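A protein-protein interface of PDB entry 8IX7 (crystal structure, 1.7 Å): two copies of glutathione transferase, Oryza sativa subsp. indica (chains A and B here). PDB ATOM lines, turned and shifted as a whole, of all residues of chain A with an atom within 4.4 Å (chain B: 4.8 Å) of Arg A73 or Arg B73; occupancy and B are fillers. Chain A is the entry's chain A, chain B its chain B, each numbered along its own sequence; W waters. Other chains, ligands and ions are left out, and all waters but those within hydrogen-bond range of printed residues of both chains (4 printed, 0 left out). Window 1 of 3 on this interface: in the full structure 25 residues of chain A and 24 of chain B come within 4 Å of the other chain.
Among the printed residues, merely in contact across the chains: Arg A69 with Glu B106, Glu A106 with Arg B69, Ala A70 with Glu B106, Arg A73 with Arg B73, Glu A106 with Ala B70, Glu A102 with Ala B70, Ala A70 with Glu B102, Glu A102 with Arg B73 and Arg A73 with Glu B102.
Arg A69 touches Glu B106, and with the chains exchanged Glu A106 touches Arg B69. Ala A70 touches Glu B102, and with the chains exchanged Glu A102 touches Ala B70. Ala A70 touches Glu B106, and with the chains exchanged Glu A106 touches Ala B70. Arg A73 touches Glu B102, and with the chains exchanged Glu A102 touches Arg B73.
Water W2 lies within hydrogen-bond range of the side-chain carboxylate of Glu A106 (2.6 Å), the guanidinium group of Arg B73 (2.9 Å) and the side-chain carboxylate of Glu B106 (2.9 Å). Water W4 bridges the side-chain carboxylate (OE1) of Glu B106 (2.7 Å) and the guanidinium group (NH1) of Arg A69 (3.0 Å). Water W1 lies within hydrogen-bond range of OE2 of Glu B106 (2.7 Å), OE2 of Glu A106 (2.9 Å) and NH2 of Arg A73 (3.0 Å). Water W3 lies within hydrogen-bond range of the side-chain carboxylate of Glu A106 (2.8 Å) and the guanidinium group of Arg B69 (2.9 Å).
Of chain B, only Arg B73 (3.7 Å), Glu B102 (3.9 Å) and Glu B106 (3.1 Å) come within 4 Å of Arg A73. Asp A77 touches none of the printed residues of chain B. Of the printed residues of chain B, Glu A106 touches Arg B69, Ala B70 and Arg B73. Printed residues of chain A within 4 Å of Ala B70: Glu A102 and Glu A106. Of the printed residues of chain A, Arg B73 touches Arg A73, Glu A102 and Glu A106. Ile B75 touches none of the printed residues of chain A. Printed residues of chain A within 4 Å of Glu B106: Arg A69 (3.5 Å), Ala A70 (3.7 Å) and Arg A73 (3.1 Å). The nearest printed residue of chain B that does not touch Arg A73 is Ala B70 (6.6 Å). The nearest printed residue of chain A that does not touch Ala B70 is Arg A73 (6.6 Å).
The guanidinium group (NH2) of Arg B73 lies within salt-bridge range of the side-chain carboxylate (OE2) of Glu B106. The backbone carbonyl oxygen (O) of Arg B69 lies close to the guanidinium group (NH1) of Arg B73, at 3.4 Å. The side-chain carboxylate of Glu B102 lies within salt-bridge range of the guanidinium group of Arg B73 (2.7 Å). The side-chain carboxylate of Glu A102 is in salt-bridge range of the guanidinium group of Arg A73 (2.7 Å). NH1 of Arg A73 lies close to O of Arg A69 (3.4 Å). The guanidinium group of Arg A73 lies within salt-bridge range of the side-chain carboxylate of Glu A106 (3.4 Å).
The guanidinium group of Arg A73 is in salt-bridge range of the side-chain carboxylate of Glu B106 (3.1 Å). OE2 of Glu A106 is in salt-bridge range of NH1 of Arg B73 (3.1 Å).
Printed residues of chain B that touch a printed residue of chain A: Arg B69, Ala B70, Arg B73, Glu B102 and Glu B106. Hydrophobic or aromatic side chains of chain B within 4 Å of the printed part of chain A: Ala B70. Printed residues of chain A that touch a printed residue of chain B: Arg A69, Ala A70, Arg A73, Glu A102 and Glu A106. Among the printed residues, 11 pairs touch across the chains. Among the printed residues, Asp or Glu carboxylates within 4 Å of a Lys or Arg side-chain nitrogen of the other chain: Arg A73 with Glu B106 (3.1 Å) and Glu A106 with Arg B73 (3.1 Å).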
ATOM      1  N   ARG A  69     -30.689 -24.184  28.482  1.00  0.00           N
ATOM      2  CA  ARG A  69     -29.439 -24.630  27.887  1.00  0.00           C
ATOM      3  C   ARG A  69     -28.540 -25.373  28.875  1.00  0.00           C
ATOM      4  O   ARG A  69     -27.786 -26.258  28.478  1.00  0.00           O
ATOM      5  CB  ARG A  69     -28.731 -23.431  27.244  1.00  0.00           C
ATOM      6  CG  ARG A  69     -29.625 -22.792  26.179  1.00  0.00           C
ATOM      7  CD  ARG A  69     -29.142 -21.429  25.702  1.00  0.00           C
ATOM      8  NE  ARG A  69     -30.160 -20.786  24.872  1.00  0.00           N
ATOM      9  CZ  ARG A  69     -31.249 -20.180  25.339  1.00  0.00           C
ATOM     10  NH1 ARG A  69     -31.481 -20.120  26.646  1.00  0.00           N
ATOM     11  NH2 ARG A  69     -32.115 -19.636  24.494  1.00  0.00           N
ATOM     12  N   ALA A  70     -28.638 -25.031  30.156  1.00  0.00           N
ATOM     13  CA  ALA A  70     -27.857 -25.708  31.186  1.00  0.00           C
ATOM     14  C   ALA A  70     -28.467 -27.098  31.388  1.00  0.00           C
ATOM     15  O   ALA A  70     -27.759 -28.091  31.548  1.00  0.00           O
ATOM     16  CB  ALA A  70     -27.905 -24.922  32.487  1.00  0.00           C
ATOM     17  N   ILE A  71     -29.794 -27.154  31.380  1.00  0.00           N
ATOM     18  CA  ILE A  71     -30.506 -28.417  31.542  1.00  0.00           C
ATOM     19  C   ILE A  71     -30.136 -29.348  30.385  1.00  0.00           C
ATOM     20  O   ILE A  71     -29.879 -30.535  30.590  1.00  0.00           O
ATOM     21  CB  ILE A  71     -32.036 -28.183  31.554  1.00  0.00           C
ATOM     22  CG1 ILE A  71     -32.422 -27.380  32.797  1.00  0.00           C
ATOM     23  CG2 ILE A  71     -32.778 -29.523  31.501  1.00  0.00           C
ATOM     24  CD1 ILE A  71     -33.841 -26.823  32.770  1.00  0.00           C
ATOM     25  N   CYS A  72     -30.101 -28.807  29.170  1.00  0.00           N
ATOM     26  CA  CYS A  72     -29.748 -29.604  28.000  1.00  0.00           C
ATOM     27  C   CYS A  72     -28.332 -30.161  28.103  1.00  0.00           C
ATOM     28  O   CYS A  72     -28.103 -31.333  27.815  1.00  0.00           O
ATOM     29  CB  CYS A  72     -29.878 -28.771  26.721  1.00  0.00           C
ATOM     30  SG  CYS A  72     -31.588 -28.508  26.201  1.00  0.00           S
ATOM     31  N   ARG A  73     -27.379 -29.328  28.509  1.00  0.00           N
ATOM     32  CA  ARG A  73     -26.004 -29.798  28.645  1.00  0.00           C
ATOM     33  C   ARG A  73     -25.920 -30.910  29.691  1.00  0.00           C
ATOM     34  O   ARG A  73     -25.189 -31.886  29.511  1.00  0.00           O
ATOM     35  CB  ARG A  73     -25.073 -28.641  29.028  1.00  0.00           C
ATOM     36  CG  ARG A  73     -24.833 -27.634  27.900  1.00  0.00           C
ATOM     37  CD  ARG A  73     -23.657 -26.720  28.237  1.00  0.00           C
ATOM     38  NE  ARG A  73     -23.330 -25.782  27.163  1.00  0.00           N
ATOM     39  CZ  ARG A  73     -24.005 -24.668  26.906  1.00  0.00           C
ATOM     40  NH1 ARG A  73     -25.058 -24.336  27.642  1.00  0.00           N
ATOM     41  NH2 ARG A  73     -23.619 -23.875  25.918  1.00  0.00           N
ATOM     42  N   TYR A  74     -26.674 -30.766  30.778  1.00  0.00           N
ATOM     43  CA  TYR A  74     -26.687 -31.772  31.836  1.00  0.00           C
ATOM     44  C   TYR A  74     -27.205 -33.102  31.295  1.00  0.00           C
ATOM     45  O   TYR A  74     -26.604 -34.158  31.514  1.00  0.00           O
ATOM     46  CB  TYR A  74     -27.587 -31.318  32.991  1.00  0.00           C
ATOM     47  CG  TYR A  74     -27.872 -32.415  33.990  1.00  0.00           C
ATOM     48  CD1 TYR A  74     -26.886 -32.858  34.872  1.00  0.00           C
ATOM     49  CD2 TYR A  74     -29.115 -33.045  34.020  1.00  0.00           C
ATOM     50  CE1 TYR A  74     -27.133 -33.911  35.760  1.00  0.00           C
ATOM     51  CE2 TYR A  74     -29.371 -34.101  34.902  1.00  0.00           C
ATOM     52  CZ  TYR A  74     -28.373 -34.528  35.766  1.00  0.00           C
ATOM     53  OH  TYR A  74     -28.611 -35.581  36.623  1.00  0.00           O
ATOM     54  N   ILE A  75     -28.326 -33.042  30.587  1.00  0.00           N
ATOM     55  CA  ILE A  75     -28.936 -34.240  30.024  1.00  0.00           C
ATOM     56  C   ILE A  75     -27.973 -34.970  29.095  1.00  0.00           C
ATOM     57  O   ILE A  75     -27.842 -36.195  29.157  1.00  0.00           O
ATOM     58  CB  ILE A  75     -30.221 -33.878  29.255  1.00  0.00           C
ATOM     59  CG1 ILE A  75     -31.250 -33.310  30.238  1.00  0.00           C
ATOM     60  CG2 ILE A  75     -30.772 -35.106  28.531  1.00  0.00           C
ATOM     61  CD1 ILE A  75     -32.458 -32.675  29.578  1.00  0.00           C
ATOM     62  N   CYS A  76     -27.289 -34.212  28.246  1.00  0.00           N
ATOM     63  CA  CYS A  76     -26.353 -34.798  27.301  1.00  0.00           C
ATOM     64  C   CYS A  76     -25.144 -35.437  27.971  1.00  0.00           C
ATOM     65  O   CYS A  76     -24.580 -36.389  27.441  1.00  0.00           O
ATOM     66  CB  CYS A  76     -25.900 -33.747  26.286  1.00  0.00           C
ATOM     67  SG  CYS A  76     -27.215 -33.260  25.144  1.00  0.00           S
ATOM     68  N   ASP A  77     -24.744 -34.920  29.129  1.00  0.00           N
ATOM     69  CA  ASP A  77     -23.598 -35.487  29.836  1.00  0.00           C
ATOM     70  C   ASP A  77     -23.990 -36.634  30.763  1.00  0.00           C
ATOM     71  O   ASP A  77     -23.300 -37.652  30.829  1.00  0.00           O
ATOM     72  CB  ASP A  77     -22.874 -34.409  30.645  1.00  0.00           C
ATOM     73  CG  ASP A  77     -22.145 -33.413  29.767  1.00  0.00           C
ATOM     74  OD1 ASP A  77     -21.470 -33.844  28.809  1.00  0.00           O
ATOM     75  OD2 ASP A  77     -22.237 -32.198  30.039  1.00  0.00           O
ATOM     76  N   GLU A 102     -20.393 -26.067  20.730  1.00  0.00           N
ATOM     77  CA  GLU A 102     -20.575 -25.005  21.712  1.00  0.00           C
ATOM     78  C   GLU A 102     -20.640 -23.589  21.140  1.00  0.00           C
ATOM     79  O   GLU A 102     -21.450 -22.781  21.591  1.00  0.00           O
ATOM     80  CB  GLU A 102     -19.465 -25.068  22.764  1.00  0.00           C
ATOM     81  CG  GLU A 102     -19.650 -26.160  23.810  1.00  0.00           C
ATOM     82  CD  GLU A 102     -20.846 -25.906  24.715  1.00  0.00           C
ATOM     83  OE1 GLU A 102     -21.351 -24.762  24.736  1.00  0.00           O
ATOM     84  OE2 GLU A 102     -21.272 -26.847  25.418  1.00  0.00           O
ATOM     85  N   ILE A 105     -24.077 -23.008  19.880  1.00  0.00           N
ATOM     86  CA  ILE A 105     -25.089 -23.017  20.927  1.00  0.00           C
ATOM     87  C   ILE A 105     -25.054 -21.604  21.507  1.00  0.00           C
ATOM     88  O   ILE A 105     -26.085 -21.011  21.819  1.00  0.00           O
ATOM     89  CB  ILE A 105     -24.762 -24.029  22.050  1.00  0.00           C
ATOM     90  CG1 ILE A 105     -24.962 -25.454  21.539  1.00  0.00           C
ATOM     91  CG2 ILE A 105     -25.643 -23.766  23.264  1.00  0.00           C
ATOM     92  CD1 ILE A 105     -24.604 -26.525  22.559  1.00  0.00           C
ATOM     93  N   GLU A 106     -23.850 -21.059  21.650  1.00  0.00           N
ATOM     94  CA  GLU A 106     -23.711 -19.707  22.175  1.00  0.00           C
ATOM     95  C   GLU A 106     -24.274 -18.686  21.186  1.00  0.00           C
ATOM     96  O   GLU A 106     -24.856 -17.679  21.590  1.00  0.00           O
ATOM     97  CB  GLU A 106     -22.244 -19.399  22.480  1.00  0.00           C
ATOM     98  CG  GLU A 106     -21.731 -20.062  23.745  1.00  0.00           C
ATOM     99  CD  GLU A 106     -22.537 -19.666  24.967  1.00  0.00           C
ATOM    100  OE1 GLU A 106     -22.787 -18.451  25.150  1.00  0.00           O
ATOM    101  OE2 GLU A 106     -22.913 -20.565  25.751  1.00  0.00           O
ATOM    102  N   ARG B  69     -18.220 -17.312  25.963  1.00  0.00           N
ATOM    103  CA  ARG B  69     -18.541 -18.414  26.859  1.00  0.00           C
ATOM    104  C   ARG B  69     -18.195 -19.790  26.284  1.00  0.00           C
ATOM    105  O   ARG B  69     -17.895 -20.722  27.035  1.00  0.00           O
ATOM    106  CB  ARG B  69     -20.010 -18.304  27.284  1.00  0.00           C
ATOM    107  CG  ARG B  69     -20.279 -16.954  27.971  1.00  0.00           C
ATOM    108  CD  ARG B  69     -21.756 -16.643  28.167  1.00  0.00           C
ATOM    109  NE  ARG B  69     -21.961 -15.255  28.600  1.00  0.00           N
ATOM    110  CZ  ARG B  69     -21.927 -14.196  27.792  1.00  0.00           C
ATOM    111  NH1 ARG B  69     -21.697 -14.347  26.494  1.00  0.00           N
ATOM    112  NH2 ARG B  69     -22.123 -12.975  28.283  1.00  0.00           N
ATOM    113  N   ALA B  70     -18.213 -19.914  24.960  1.00  0.00           N
ATOM    114  CA  ALA B  70     -17.851 -21.175  24.316  1.00  0.00           C
ATOM    115  C   ALA B  70     -16.328 -21.287  24.413  1.00  0.00           C
ATOM    116  O   ALA B  70     -15.781 -22.361  24.661  1.00  0.00           O
ATOM    117  CB  ALA B  70     -18.290 -21.172  22.855  1.00  0.00           C
ATOM    118  N   ILE B  71     -15.645 -20.163  24.207  1.00  0.00           N
ATOM    119  CA  ILE B  71     -14.189 -20.132  24.297  1.00  0.00           C
ATOM    120  C   ILE B  71     -13.774 -20.554  25.704  1.00  0.00           C
ATOM    121  O   ILE B  71     -12.855 -21.357  25.874  1.00  0.00           O
ATOM    122  CB  ILE B  71     -13.636 -18.712  24.011  1.00  0.00           C
ATOM    123  CG1 ILE B  71     -13.882 -18.342  22.549  1.00  0.00           C
ATOM    124  CG2 ILE B  71     -12.133 -18.653  24.331  1.00  0.00           C
ATOM    125  CD1 ILE B  71     -13.697 -16.860  22.258  1.00  0.00           C
ATOM    126  N   CYS B  72     -14.452 -20.013  26.714  1.00  0.00           N
ATOM    127  CA  CYS B  72     -14.141 -20.352  28.099  1.00  0.00           C
ATOM    128  C   CYS B  72     -14.344 -21.837  28.380  1.00  0.00           C
ATOM    129  O   CYS B  72     -13.514 -22.469  29.033  1.00  0.00           O
ATOM    130  CB  CYS B  72     -14.998 -19.527  29.066  1.00  0.00           C
ATOM    131  SG  CYS B  72     -14.496 -17.793  29.208  1.00  0.00           S
ATOM    132  N   ARG B  73     -15.445 -22.399  27.894  1.00  0.00           N
ATOM    133  CA  ARG B  73     -15.700 -23.816  28.120  1.00  0.00           C
ATOM    134  C   ARG B  73     -14.619 -24.662  27.456  1.00  0.00           C
ATOM    135  O   ARG B  73     -14.189 -25.676  28.006  1.00  0.00           O
ATOM    136  CB  ARG B  73     -17.086 -24.210  27.594  1.00  0.00           C
ATOM    137  CG  ARG B  73     -18.248 -23.656  28.426  1.00  0.00           C
ATOM    138  CD  ARG B  73     -19.549 -24.387  28.108  1.00  0.00           C
ATOM    139  NE  ARG B  73     -20.685 -23.895  28.886  1.00  0.00           N
ATOM    140  CZ  ARG B  73     -21.335 -22.762  28.634  1.00  0.00           C
ATOM    141  NH1 ARG B  73     -20.962 -21.994  27.620  1.00  0.00           N
ATOM    142  NH2 ARG B  73     -22.371 -22.407  29.384  1.00  0.00           N
ATOM    143  N   TYR B  74     -14.175 -24.238  26.277  1.00  0.00           N
ATOM    144  CA  TYR B  74     -13.132 -24.953  25.547  1.00  0.00           C
ATOM    145  C   TYR B  74     -11.832 -24.938  26.352  1.00  0.00           C
ATOM    146  O   TYR B  74     -11.184 -25.970  26.535  1.00  0.00           O
ATOM    147  CB  TYR B  74     -12.895 -24.298  24.181  1.00  0.00           C
ATOM    148  CG  TYR B  74     -11.687 -24.855  23.453  1.00  0.00           C
ATOM    149  CD1 TYR B  74     -11.712 -26.128  22.887  1.00  0.00           C
ATOM    150  CD2 TYR B  74     -10.498 -24.132  23.393  1.00  0.00           C
ATOM    151  CE1 TYR B  74     -10.578 -26.672  22.284  1.00  0.00           C
ATOM    152  CE2 TYR B  74      -9.355 -24.666  22.797  1.00  0.00           C
ATOM    153  CZ  TYR B  74      -9.403 -25.935  22.247  1.00  0.00           C
ATOM    154  OH  TYR B  74      -8.273 -26.468  21.672  1.00  0.00           O
ATOM    155  N   ILE B  75     -11.450 -23.759  26.829  1.00  0.00           N
ATOM    156  CA  ILE B  75     -10.228 -23.625  27.613  1.00  0.00           C
ATOM    157  C   ILE B  75     -10.259 -24.522  28.855  1.00  0.00           C
ATOM    158  O   ILE B  75      -9.303 -25.244  29.134  1.00  0.00           O
ATOM    159  CB  ILE B  75     -10.013 -22.152  28.034  1.00  0.00           C
ATOM    160  CG1 ILE B  75      -9.778 -21.295  26.783  1.00  0.00           C
ATOM    161  CG2 ILE B  75      -8.826 -22.046  28.985  1.00  0.00           C
ATOM    162  CD1 ILE B  75      -9.882 -19.790  27.020  1.00  0.00           C
ATOM    163  N   CYS B  76     -11.363 -24.489  29.592  1.00  0.00           N
ATOM    164  CA  CYS B  76     -11.488 -25.299  30.799  1.00  0.00           C
ATOM    165  C   CYS B  76     -11.402 -26.802  30.577  1.00  0.00           C
ATOM    166  O   CYS B  76     -10.887 -27.524  31.427  1.00  0.00           O
ATOM    167  CB  CYS B  76     -12.796 -24.981  31.522  1.00  0.00           C
ATOM    168  SG  CYS B  76     -12.823 -23.361  32.300  1.00  0.00           S
ATOM    169  N   ASP B  77     -11.905 -27.287  29.449  1.00  0.00           N
ATOM    170  CA  ASP B  77     -11.860 -28.722  29.207  1.00  0.00           C
ATOM    171  C   ASP B  77     -10.590 -29.176  28.496  1.00  0.00           C
ATOM    172  O   ASP B  77     -10.064 -30.250  28.781  1.00  0.00           O
ATOM    173  CB  ASP B  77     -13.099 -29.170  28.421  1.00  0.00           C
ATOM    174  CG  ASP B  77     -14.388 -29.007  29.219  1.00  0.00           C
ATOM    175  OD1 ASP B  77     -14.356 -29.143  30.463  1.00  0.00           O
ATOM    176  OD2 ASP B  77     -15.443 -28.759  28.600  1.00  0.00           O
ATOM    177  N   GLU B 102     -23.057 -24.635  35.545  1.00  0.00           N
ATOM    178  CA  GLU B 102     -23.700 -24.255  34.292  1.00  0.00           C
ATOM    179  C   GLU B 102     -24.981 -23.435  34.424  1.00  0.00           C
ATOM    180  O   GLU B 102     -25.212 -22.508  33.642  1.00  0.00           O
ATOM    181  CB  GLU B 102     -23.987 -25.506  33.456  1.00  0.00           C
ATOM    182  CG  GLU B 102     -22.760 -26.106  32.789  1.00  0.00           C
ATOM    183  CD  GLU B 102     -22.260 -25.260  31.629  1.00  0.00           C
ATOM    184  OE1 GLU B 102     -22.945 -24.277  31.268  1.00  0.00           O
ATOM    185  OE2 GLU B 102     -21.190 -25.583  31.073  1.00  0.00           O
ATOM    186  N   ILE B 105     -24.008 -19.951  34.863  1.00  0.00           N
ATOM    187  CA  ILE B 105     -23.320 -19.390  33.702  1.00  0.00           C
ATOM    188  C   ILE B 105     -24.452 -18.947  32.780  1.00  0.00           C
ATOM    189  O   ILE B 105     -24.386 -17.903  32.142  1.00  0.00           O
ATOM    190  CB  ILE B 105     -22.454 -20.442  32.959  1.00  0.00           C
ATOM    191  CG1 ILE B 105     -21.238 -20.827  33.807  1.00  0.00           C
ATOM    192  CG2 ILE B 105     -21.990 -19.876  31.621  1.00  0.00           C
ATOM    193  CD1 ILE B 105     -20.395 -21.938  33.194  1.00  0.00           C
ATOM    194  N   GLU B 106     -25.509 -19.753  32.726  1.00  0.00           N
ATOM    195  CA  GLU B 106     -26.656 -19.423  31.895  1.00  0.00           C
ATOM    196  C   GLU B 106     -27.398 -18.209  32.447  1.00  0.00           C
ATOM    197  O   GLU B 106     -27.896 -17.380  31.685  1.00  0.00           O
ATOM    198  CB  GLU B 106     -27.600 -20.621  31.796  1.00  0.00           C
ATOM    199  CG  GLU B 106     -27.080 -21.727  30.897  1.00  0.00           C
ATOM    200  CD  GLU B 106     -26.804 -21.254  29.472  1.00  0.00           C
ATOM    201  OE1 GLU B 106     -27.660 -20.556  28.888  1.00  0.00           O
ATOM    202  OE2 GLU B 106     -25.733 -21.593  28.931  1.00  0.00           O
ATOM    203  N   LEU B 169     -16.267 -21.092  37.083  1.00  0.00           N
ATOM    204  CA  LEU B 169     -16.484 -20.301  35.878  1.00  0.00           C
ATOM    205  C   LEU B 169     -17.779 -19.498  36.037  1.00  0.00           C
ATOM    206  O   LEU B 169     -17.946 -18.452  35.410  1.00  0.00           O
ATOM    207  CB  LEU B 169     -16.556 -21.222  34.653  1.00  0.00           C
ATOM    208  CG  LEU B 169     -16.689 -20.560  33.276  1.00  0.00           C
ATOM    209  CD1 LEU B 169     -15.496 -19.629  33.034  1.00  0.00           C
ATOM    210  CD2 LEU B 169     -16.764 -21.634  32.196  1.00  0.00           C
HETATM  211  O   HOH W   1     -25.570 -21.567  26.244  1.00  0.00           O
HETATM  212  O   HOH W   2     -23.417 -19.941  28.270  1.00  0.00           O
HETATM  213  O   HOH W   3     -20.827 -16.476  24.698  1.00  0.00           O
HETATM  214  O   HOH W   4     -30.229 -21.272  29.114  1.00  0.00           O
